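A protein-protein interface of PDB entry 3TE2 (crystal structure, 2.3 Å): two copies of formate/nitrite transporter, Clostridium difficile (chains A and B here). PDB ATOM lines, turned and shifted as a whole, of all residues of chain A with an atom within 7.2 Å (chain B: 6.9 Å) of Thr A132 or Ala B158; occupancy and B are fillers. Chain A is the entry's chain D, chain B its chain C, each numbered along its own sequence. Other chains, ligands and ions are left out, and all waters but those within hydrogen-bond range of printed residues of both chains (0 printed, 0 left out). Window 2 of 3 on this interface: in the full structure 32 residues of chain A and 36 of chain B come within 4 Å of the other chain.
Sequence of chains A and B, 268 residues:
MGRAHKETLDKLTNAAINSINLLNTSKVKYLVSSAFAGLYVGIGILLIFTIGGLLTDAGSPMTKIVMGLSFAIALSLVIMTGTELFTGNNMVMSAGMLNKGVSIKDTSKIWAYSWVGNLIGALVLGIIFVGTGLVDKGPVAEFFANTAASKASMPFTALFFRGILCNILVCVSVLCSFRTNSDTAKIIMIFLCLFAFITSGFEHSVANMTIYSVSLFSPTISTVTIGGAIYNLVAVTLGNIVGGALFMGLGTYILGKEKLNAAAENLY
Of the 11 printed residues of chain A, 5 touch a printed residue of chain B.
Hydrophobic or aromatic side chains of chain A within 4 Å of the printed part of chain B: Ile A128 and Leu A134.
Along chain A the printed residues that touch a printed residue of chain B span positions 128 to 134.
Printed residues of chain B that touch a printed residue of chain A: Thr B157, Ala B158, Phe B161, Arg B162, Leu B165, Ser B200 and Phe B202.
Along chain B the printed residues that touch a printed residue of chain A span positions 157 to 202.
Among the printed residues, 12 pairs touch across the chains.
Among the printed residues, no Asp or Glu carboxylate lies within 4 Å of a Lys or Arg side-chain nitrogen of the other chain.
Phe B161 touches Ile A128 (CB to O, 3.7 Å).
Leu B165 touches Phe A129.
O of Thr B157 touches O of Gly A131, at 3.8 Å.
O of Gly A131 touches CA of Ala B158, 3.7 Å away.
Gly A131 touches Phe B161 (O to CD2, 3.4 Å).
Ala B158 touches Thr A132 (CB to O, 3.3 Å).
Thr A132 touches Phe B161.
Leu A134 touches Arg B162.
Ser B200 touches Leu A134.
CD1 of Leu A134 touches CE1 of Phe B202, at 3.8 Å.
No position is printed for both chains.
Of the 12 pairs that touch across the chains among the printed residues, none has its exchanged pair printed and touching as well.
Printed residues of chain B within 4 Å of Phe A129: Leu B165 (3.97 Å).
Of chain B, only Thr B157, Ala B158 and Phe B161 come within 4 Å of Gly A131.
Thr A132 touches just these residues of chain B: Ala B158 (3.3 Å), Phe B161 (3.6 Å) and Arg B162 (3.0 Å).
Of the printed residues of chain B, Leu A134 touches Arg B162 (3.5 Å), Ser B200 (3.2 Å) and Phe B202 (3.8 Å).
Of the printed residues of chain A, Ala B158 touches Gly A131 (3.7 Å) and Thr A132 (3.3 Å).
Of the printed residues of chain A, Phe B202 touches Leu A134 (3.8 Å).
The guanidinium group (NE) of Arg B162 lies within hydrogen-bond range of the backbone carbonyl oxygen (O) of Thr A132, at 3.0 Å.
N of Glu B203 sits at hydrogen-bond distance from O of Arg B162, 3.1 Å away.
NH1 of Arg B162 sits close to SD of Met B154.
OG1 of Thr A132 sits close to N of Leu A134.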
ATOM      1  N   GLY A 126      -0.938   2.499   4.532  1.00  0.00           N
ATOM      2  CA  GLY A 126       0.123   1.630   4.056  1.00  0.00           C
ATOM      3  C   GLY A 126       0.608   2.036   2.678  1.00  0.00           C
ATOM      4  O   GLY A 126       1.811   2.071   2.416  1.00  0.00           O
ATOM      5  N   ILE A 127      -0.338   2.343   1.796  1.00  0.00           N
ATOM      6  CA  ILE A 127      -0.019   2.781   0.445  1.00  0.00           C
ATOM      7  C   ILE A 127       0.807   4.061   0.479  1.00  0.00           C
ATOM      8  O   ILE A 127       1.864   4.149  -0.149  1.00  0.00           O
ATOM      9  CB  ILE A 127      -1.298   3.026  -0.383  1.00  0.00           C
ATOM     10  CG1 ILE A 127      -1.979   1.700  -0.723  1.00  0.00           C
ATOM     11  CG2 ILE A 127      -0.977   3.796  -1.649  1.00  0.00           C
ATOM     12  CD1 ILE A 127      -3.230   1.849  -1.563  1.00  0.00           C
ATOM     13  N   ILE A 128       0.321   5.049   1.222  1.00  0.00           N
ATOM     14  CA  ILE A 128       0.989   6.340   1.300  1.00  0.00           C
ATOM     15  C   ILE A 128       2.371   6.234   1.936  1.00  0.00           C
ATOM     16  O   ILE A 128       3.320   6.865   1.469  1.00  0.00           O
ATOM     17  CB  ILE A 128       0.145   7.363   2.078  1.00  0.00           C
ATOM     18  CG1 ILE A 128      -1.192   7.593   1.369  1.00  0.00           C
ATOM     19  CG2 ILE A 128       0.909   8.672   2.237  1.00  0.00           C
ATOM     20  CD1 ILE A 128      -2.147   8.468   2.148  1.00  0.00           C
ATOM     21  N   PHE A 129       2.479   5.437   2.998  1.00  0.00           N
ATOM     22  CA  PHE A 129       3.758   5.235   3.681  1.00  0.00           C
ATOM     23  C   PHE A 129       4.806   4.655   2.729  1.00  0.00           C
ATOM     24  O   PHE A 129       5.901   5.205   2.590  1.00  0.00           O
ATOM     25  CB  PHE A 129       3.587   4.335   4.911  1.00  0.00           C
ATOM     26  CG  PHE A 129       4.834   4.203   5.750  1.00  0.00           C
ATOM     27  CD1 PHE A 129       5.456   5.325   6.273  1.00  0.00           C
ATOM     28  CD2 PHE A 129       5.374   2.958   6.025  1.00  0.00           C
ATOM     29  CE1 PHE A 129       6.597   5.208   7.051  1.00  0.00           C
ATOM     30  CE2 PHE A 129       6.515   2.833   6.799  1.00  0.00           C
ATOM     31  CZ  PHE A 129       7.128   3.960   7.312  1.00  0.00           C
ATOM     32  N   VAL A 130       4.466   3.549   2.075  1.00  0.00           N
ATOM     33  CA  VAL A 130       5.337   2.960   1.058  1.00  0.00           C
ATOM     34  C   VAL A 130       5.775   3.999   0.024  1.00  0.00           C
ATOM     35  O   VAL A 130       6.921   3.993  -0.426  1.00  0.00           O
ATOM     36  CB  VAL A 130       4.653   1.781   0.344  1.00  0.00           C
ATOM     37  CG1 VAL A 130       5.407   1.410  -0.937  1.00  0.00           C
ATOM     38  CG2 VAL A 130       4.552   0.587   1.281  1.00  0.00           C
ATOM     39  N   GLY A 131       4.864   4.900  -0.333  1.00  0.00           N
ATOM     40  CA  GLY A 131       5.155   5.951  -1.293  1.00  0.00           C
ATOM     41  C   GLY A 131       6.199   6.959  -0.835  1.00  0.00           C
ATOM     42  O   GLY A 131       6.745   7.705  -1.651  1.00  0.00           O
ATOM     43  N   THR A 132       6.475   6.993   0.467  1.00  0.00           N
ATOM     44  CA  THR A 132       7.498   7.889   1.002  1.00  0.00           C
ATOM     45  C   THR A 132       8.888   7.325   0.754  1.00  0.00           C
ATOM     46  O   THR A 132       9.876   8.056   0.781  1.00  0.00           O
ATOM     47  CB  THR A 132       7.339   8.104   2.518  1.00  0.00           C
ATOM     48  OG1 THR A 132       7.484   6.851   3.197  1.00  0.00           O
ATOM     49  CG2 THR A 132       5.978   8.701   2.837  1.00  0.00           C
ATOM     50  N   GLY A 133       8.952   6.016   0.520  1.00  0.00           N
ATOM     51  CA  GLY A 133      10.213   5.334   0.293  1.00  0.00           C
ATOM     52  C   GLY A 133      10.934   4.982   1.580  1.00  0.00           C
ATOM     53  O   GLY A 133      12.062   4.488   1.549  1.00  0.00           O
ATOM     54  N   LEU A 134      10.280   5.229   2.714  1.00  0.00           N
ATOM     55  CA  LEU A 134      10.881   4.978   4.024  1.00  0.00           C
ATOM     56  C   LEU A 134      11.109   3.493   4.321  1.00  0.00           C
ATOM     57  O   LEU A 134      11.947   3.141   5.152  1.00  0.00           O
ATOM     58  CB  LEU A 134      10.048   5.629   5.135  1.00  0.00           C
ATOM     59  CG  LEU A 134      10.147   7.156   5.177  1.00  0.00           C
ATOM     60  CD1 LEU A 134       9.077   7.754   6.063  1.00  0.00           C
ATOM     61  CD2 LEU A 134      11.535   7.591   5.628  1.00  0.00           C
ATOM     62  N   VAL A 135      10.365   2.622   3.646  1.00  0.00           N
ATOM     63  CA  VAL A 135      10.591   1.188   3.790  1.00  0.00           C
ATOM     64  C   VAL A 135      11.144   0.575   2.502  1.00  0.00           C
ATOM     65  O   VAL A 135      11.016  -0.630   2.269  1.00  0.00           O
ATOM     66  CB  VAL A 135       9.317   0.434   4.254  1.00  0.00           C
ATOM     67  CG1 VAL A 135       8.993   0.780   5.703  1.00  0.00           C
ATOM     68  CG2 VAL A 135       8.141   0.754   3.348  1.00  0.00           C
ATOM     69  N   ASP A 136      11.762   1.411   1.671  1.00  0.00           N
ATOM     70  CA  ASP A 136      12.450   0.921   0.479  1.00  0.00           C
ATOM     71  C   ASP A 136      13.536  -0.078   0.867  1.00  0.00           C
ATOM     72  O   ASP A 136      13.664  -1.132   0.250  1.00  0.00           O
ATOM     73  CB  ASP A 136      13.050   2.073  -0.337  1.00  0.00           C
ATOM     74  CG  ASP A 136      12.044   2.712  -1.284  1.00  0.00           C
ATOM     75  OD1 ASP A 136      10.962   2.122  -1.493  1.00  0.00           O
ATOM     76  OD2 ASP A 136      12.337   3.797  -1.831  1.00  0.00           O
ATOM     77  N   MET B 154      16.291  14.592  -2.734  1.00  0.00           N
ATOM     78  CA  MET B 154      15.407  13.432  -2.646  1.00  0.00           C
ATOM     79  C   MET B 154      14.337  13.483  -3.733  1.00  0.00           C
ATOM     80  O   MET B 154      13.815  14.553  -4.043  1.00  0.00           O
ATOM     81  CB  MET B 154      14.761  13.347  -1.257  1.00  0.00           C
ATOM     82  CG  MET B 154      13.654  12.301  -1.135  1.00  0.00           C
ATOM     83  SD  MET B 154      13.131  11.986   0.570  1.00  0.00           S
ATOM     84  CE  MET B 154      14.567  11.130   1.212  1.00  0.00           C
ATOM     85  N   PRO B 155      14.010  12.320  -4.321  1.00  0.00           N
ATOM     86  CA  PRO B 155      13.012  12.219  -5.393  1.00  0.00           C
ATOM     87  C   PRO B 155      11.689  12.891  -5.029  1.00  0.00           C
ATOM     88  O   PRO B 155      11.299  12.909  -3.859  1.00  0.00           O
ATOM     89  CB  PRO B 155      12.818  10.708  -5.540  1.00  0.00           C
ATOM     90  CG  PRO B 155      14.123  10.129  -5.120  1.00  0.00           C
ATOM     91  CD  PRO B 155      14.613  11.015  -4.002  1.00  0.00           C
ATOM     92  N   PHE B 156      11.006  13.428  -6.035  1.00  0.00           N
ATOM     93  CA  PHE B 156       9.787  14.204  -5.820  1.00  0.00           C
ATOM     94  C   PHE B 156       8.671  13.402  -5.161  1.00  0.00           C
ATOM     95  O   PHE B 156       8.070  13.851  -4.185  1.00  0.00           O
ATOM     96  CB  PHE B 156       9.283  14.786  -7.141  1.00  0.00           C
ATOM     97  CG  PHE B 156       8.029  15.600  -7.000  1.00  0.00           C
ATOM     98  CD1 PHE B 156       6.794  14.981  -6.912  1.00  0.00           C
ATOM     99  CD2 PHE B 156       8.086  16.983  -6.944  1.00  0.00           C
ATOM    100  CE1 PHE B 156       5.637  15.725  -6.779  1.00  0.00           C
ATOM    101  CE2 PHE B 156       6.932  17.733  -6.812  1.00  0.00           C
ATOM    102  CZ  PHE B 156       5.706  17.103  -6.730  1.00  0.00           C
ATOM    103  N   THR B 157       8.387  12.225  -5.710  1.00  0.00           N
ATOM    104  CA  THR B 157       7.327  11.369  -5.188  1.00  0.00           C
ATOM    105  C   THR B 157       7.492  11.130  -3.693  1.00  0.00           C
ATOM    106  O   THR B 157       6.532  11.228  -2.927  1.00  0.00           O
ATOM    107  CB  THR B 157       7.300  10.007  -5.905  1.00  0.00           C
ATOM    108  OG1 THR B 157       6.955  10.198  -7.282  1.00  0.00           O
ATOM    109  CG2 THR B 157       6.280   9.081  -5.254  1.00  0.00           C
ATOM    110  N   ALA B 158       8.718  10.814  -3.287  1.00  0.00           N
ATOM    111  CA  ALA B 158       9.020  10.571  -1.885  1.00  0.00           C
ATOM    112  C   ALA B 158       8.705  11.808  -1.045  1.00  0.00           C
ATOM    113  O   ALA B 158       7.970  11.728  -0.061  1.00  0.00           O
ATOM    114  CB  ALA B 158      10.472  10.158  -1.719  1.00  0.00           C
ATOM    115  N   LEU B 159       9.258  12.950  -1.443  1.00  0.00           N
ATOM    116  CA  LEU B 159       9.001  14.208  -0.743  1.00  0.00           C
ATOM    117  C   LEU B 159       7.511  14.513  -0.681  1.00  0.00           C
ATOM    118  O   LEU B 159       7.012  15.011   0.328  1.00  0.00           O
ATOM    119  CB  LEU B 159       9.734  15.366  -1.421  1.00  0.00           C
ATOM    120  CG  LEU B 159      11.253  15.398  -1.251  1.00  0.00           C
ATOM    121  CD1 LEU B 159      11.857  16.526  -2.077  1.00  0.00           C
ATOM    122  CD2 LEU B 159      11.619  15.539   0.216  1.00  0.00           C
ATOM    123  N   PHE B 160       6.809  14.210  -1.768  1.00  0.00           N
ATOM    124  CA  PHE B 160       5.381  14.489  -1.863  1.00  0.00           C
ATOM    125  C   PHE B 160       4.606  13.712  -0.807  1.00  0.00           C
ATOM    126  O   PHE B 160       3.834  14.284  -0.035  1.00  0.00           O
ATOM    127  CB  PHE B 160       4.865  14.150  -3.266  1.00  0.00           C
ATOM    128  CG  PHE B 160       3.369  14.261  -3.411  1.00  0.00           C
ATOM    129  CD1 PHE B 160       2.753  15.500  -3.470  1.00  0.00           C
ATOM    130  CD2 PHE B 160       2.582  13.123  -3.508  1.00  0.00           C
ATOM    131  CE1 PHE B 160       1.379  15.603  -3.612  1.00  0.00           C
ATOM    132  CE2 PHE B 160       1.208  13.220  -3.650  1.00  0.00           C
ATOM    133  CZ  PHE B 160       0.606  14.461  -3.704  1.00  0.00           C
ATOM    134  N   PHE B 161       4.824  12.403  -0.774  1.00  0.00           N
ATOM    135  CA  PHE B 161       4.119  11.549   0.166  1.00  0.00           C
ATOM    136  C   PHE B 161       4.521  11.814   1.618  1.00  0.00           C
ATOM    137  O   PHE B 161       3.710  11.659   2.527  1.00  0.00           O
ATOM    138  CB  PHE B 161       4.292  10.074  -0.206  1.00  0.00           C
ATOM    139  CG  PHE B 161       3.470   9.658  -1.392  1.00  0.00           C
ATOM    140  CD1 PHE B 161       2.112   9.409  -1.255  1.00  0.00           C
ATOM    141  CD2 PHE B 161       4.046   9.527  -2.643  1.00  0.00           C
ATOM    142  CE1 PHE B 161       1.346   9.032  -2.343  1.00  0.00           C
ATOM    143  CE2 PHE B 161       3.285   9.147  -3.737  1.00  0.00           C
ATOM    144  CZ  PHE B 161       1.934   8.901  -3.587  1.00  0.00           C
ATOM    145  N   ARG B 162       5.765  12.223   1.837  1.00  0.00           N
ATOM    146  CA  ARG B 162       6.198  12.570   3.187  1.00  0.00           C
ATOM    147  C   ARG B 162       5.503  13.846   3.650  1.00  0.00           C
ATOM    148  O   ARG B 162       5.232  14.020   4.838  1.00  0.00           O
ATOM    149  CB  ARG B 162       7.720  12.703   3.263  1.00  0.00           C
ATOM    150  CG  ARG B 162       8.440  11.401   2.952  1.00  0.00           C
ATOM    151  CD  ARG B 162       9.934  11.482   3.213  1.00  0.00           C
ATOM    152  NE  ARG B 162      10.620  10.297   2.703  1.00  0.00           N
ATOM    153  CZ  ARG B 162      11.878   9.976   2.984  1.00  0.00           C
ATOM    154  NH1 ARG B 162      12.600  10.748   3.788  1.00  0.00           N
ATOM    155  NH2 ARG B 162      12.412   8.875   2.467  1.00  0.00           N
ATOM    156  N   GLY B 163       5.203  14.726   2.698  1.00  0.00           N
ATOM    157  CA  GLY B 163       4.464  15.941   2.987  1.00  0.00           C
ATOM    158  C   GLY B 163       3.038  15.634   3.399  1.00  0.00           C
ATOM    159  O   GLY B 163       2.507  16.233   4.334  1.00  0.00           O
ATOM    160  N   ILE B 164       2.418  14.690   2.697  1.00  0.00           N
ATOM    161  CA  ILE B 164       1.062  14.253   3.011  1.00  0.00           C
ATOM    162  C   ILE B 164       0.939  13.787   4.461  1.00  0.00           C
ATOM    163  O   ILE B 164       0.122  14.306   5.229  1.00  0.00           O
ATOM    164  CB  ILE B 164       0.614  13.108   2.082  1.00  0.00           C
ATOM    165  CG1 ILE B 164       0.377  13.635   0.661  1.00  0.00           C
ATOM    166  CG2 ILE B 164      -0.634  12.431   2.631  1.00  0.00           C
ATOM    167  CD1 ILE B 164      -0.140  12.586  -0.313  1.00  0.00           C
ATOM    168  N   LEU B 165       1.761  12.808   4.833  1.00  0.00           N
ATOM    169  CA  LEU B 165       1.691  12.228   6.170  1.00  0.00           C
ATOM    170  C   LEU B 165       2.060  13.234   7.251  1.00  0.00           C
ATOM    171  O   LEU B 165       1.527  13.185   8.361  1.00  0.00           O
ATOM    172  CB  LEU B 165       2.574  10.980   6.271  1.00  0.00           C
ATOM    173  CG  LEU B 165       2.106   9.809   5.406  1.00  0.00           C
ATOM    174  CD1 LEU B 165       2.919   8.552   5.687  1.00  0.00           C
ATOM    175  CD2 LEU B 165       0.627   9.552   5.643  1.00  0.00           C
ATOM    176  N   SER B 200       9.399   9.460  12.466  1.00  0.00           N
ATOM    177  CA  SER B 200       9.044   8.613  11.329  1.00  0.00           C
ATOM    178  C   SER B 200       9.704   9.090  10.035  1.00  0.00           C
ATOM    179  O   SER B 200       9.971   8.288   9.138  1.00  0.00           O
ATOM    180  CB  SER B 200       7.526   8.542  11.154  1.00  0.00           C
ATOM    181  OG  SER B 200       6.908   7.985  12.303  1.00  0.00           O
ATOM    182  N   GLY B 201       9.959  10.393   9.940  1.00  0.00           N
ATOM    183  CA  GLY B 201      10.674  10.942   8.799  1.00  0.00           C
ATOM    184  C   GLY B 201       9.823  11.648   7.755  1.00  0.00           C
ATOM    185  O   GLY B 201      10.152  11.633   6.569  1.00  0.00           O
ATOM    186  N   PHE B 202       8.733  12.276   8.191  1.00  0.00           N
ATOM    187  CA  PHE B 202       7.848  13.002   7.280  1.00  0.00           C
ATOM    188  C   PHE B 202       8.323  14.444   7.099  1.00  0.00           C
ATOM    189  O   PHE B 202       9.115  14.947   7.895  1.00  0.00           O
ATOM    190  CB  PHE B 202       6.404  12.952   7.782  1.00  0.00           C
ATOM    191  CG  PHE B 202       5.918  11.558   8.074  1.00  0.00           C
ATOM    192  CD1 PHE B 202       6.404  10.476   7.353  1.00  0.00           C
ATOM    193  CD2 PHE B 202       4.992  11.324   9.078  1.00  0.00           C
ATOM    194  CE1 PHE B 202       5.968   9.186   7.620  1.00  0.00           C
ATOM    195  CE2 PHE B 202       4.554  10.036   9.352  1.00  0.00           C
ATOM    196  CZ  PHE B 202       5.043   8.966   8.620  1.00  0.00           C
ATOM    197  N   GLU B 203       7.841  15.104   6.052  1.00  0.00           N
ATOM    198  CA  GLU B 203       8.365  16.414   5.669  1.00  0.00           C
ATOM    199  C   GLU B 203       7.375  17.559   5.896  1.00  0.00           C
ATOM    200  O   GLU B 203       6.233  17.511   5.430  1.00  0.00           O
ATOM    201  CB  GLU B 203       8.816  16.384   4.207  1.00  0.00           C
ATOM    202  CG  GLU B 203       9.943  15.397   3.918  1.00  0.00           C
ATOM    203  CD  GLU B 203      11.330  15.994   4.140  1.00  0.00           C
ATOM    204  OE1 GLU B 203      11.485  17.228   4.003  1.00  0.00           O
ATOM    205  OE2 GLU B 203      12.268  15.225   4.447  1.00  0.00           O
ATOM    206  N   TYR B 231      12.937  23.420  -4.929  1.00  0.00           N
ATOM    207  CA  TYR B 231      12.480  22.071  -5.236  1.00  0.00           C
ATOM    208  C   TYR B 231      11.792  21.455  -4.024  1.00  0.00           C
ATOM    209  O   TYR B 231      10.583  21.223  -4.034  1.00  0.00           O
ATOM    210  CB  TYR B 231      13.654  21.196  -5.678  1.00  0.00           C
ATOM    211  CG  TYR B 231      13.313  19.729  -5.801  1.00  0.00           C
ATOM    212  CD1 TYR B 231      12.193  19.313  -6.507  1.00  0.00           C
ATOM    213  CD2 TYR B 231      14.112  18.758  -5.210  1.00  0.00           C
ATOM    214  CE1 TYR B 231      11.877  17.972  -6.621  1.00  0.00           C
ATOM    215  CE2 TYR B 231      13.805  17.416  -5.319  1.00  0.00           C
ATOM    216  CZ  TYR B 231      12.687  17.028  -6.026  1.00  0.00           C
ATOM    217  OH  TYR B 231      12.376  15.693  -6.137  1.00  0.00           O
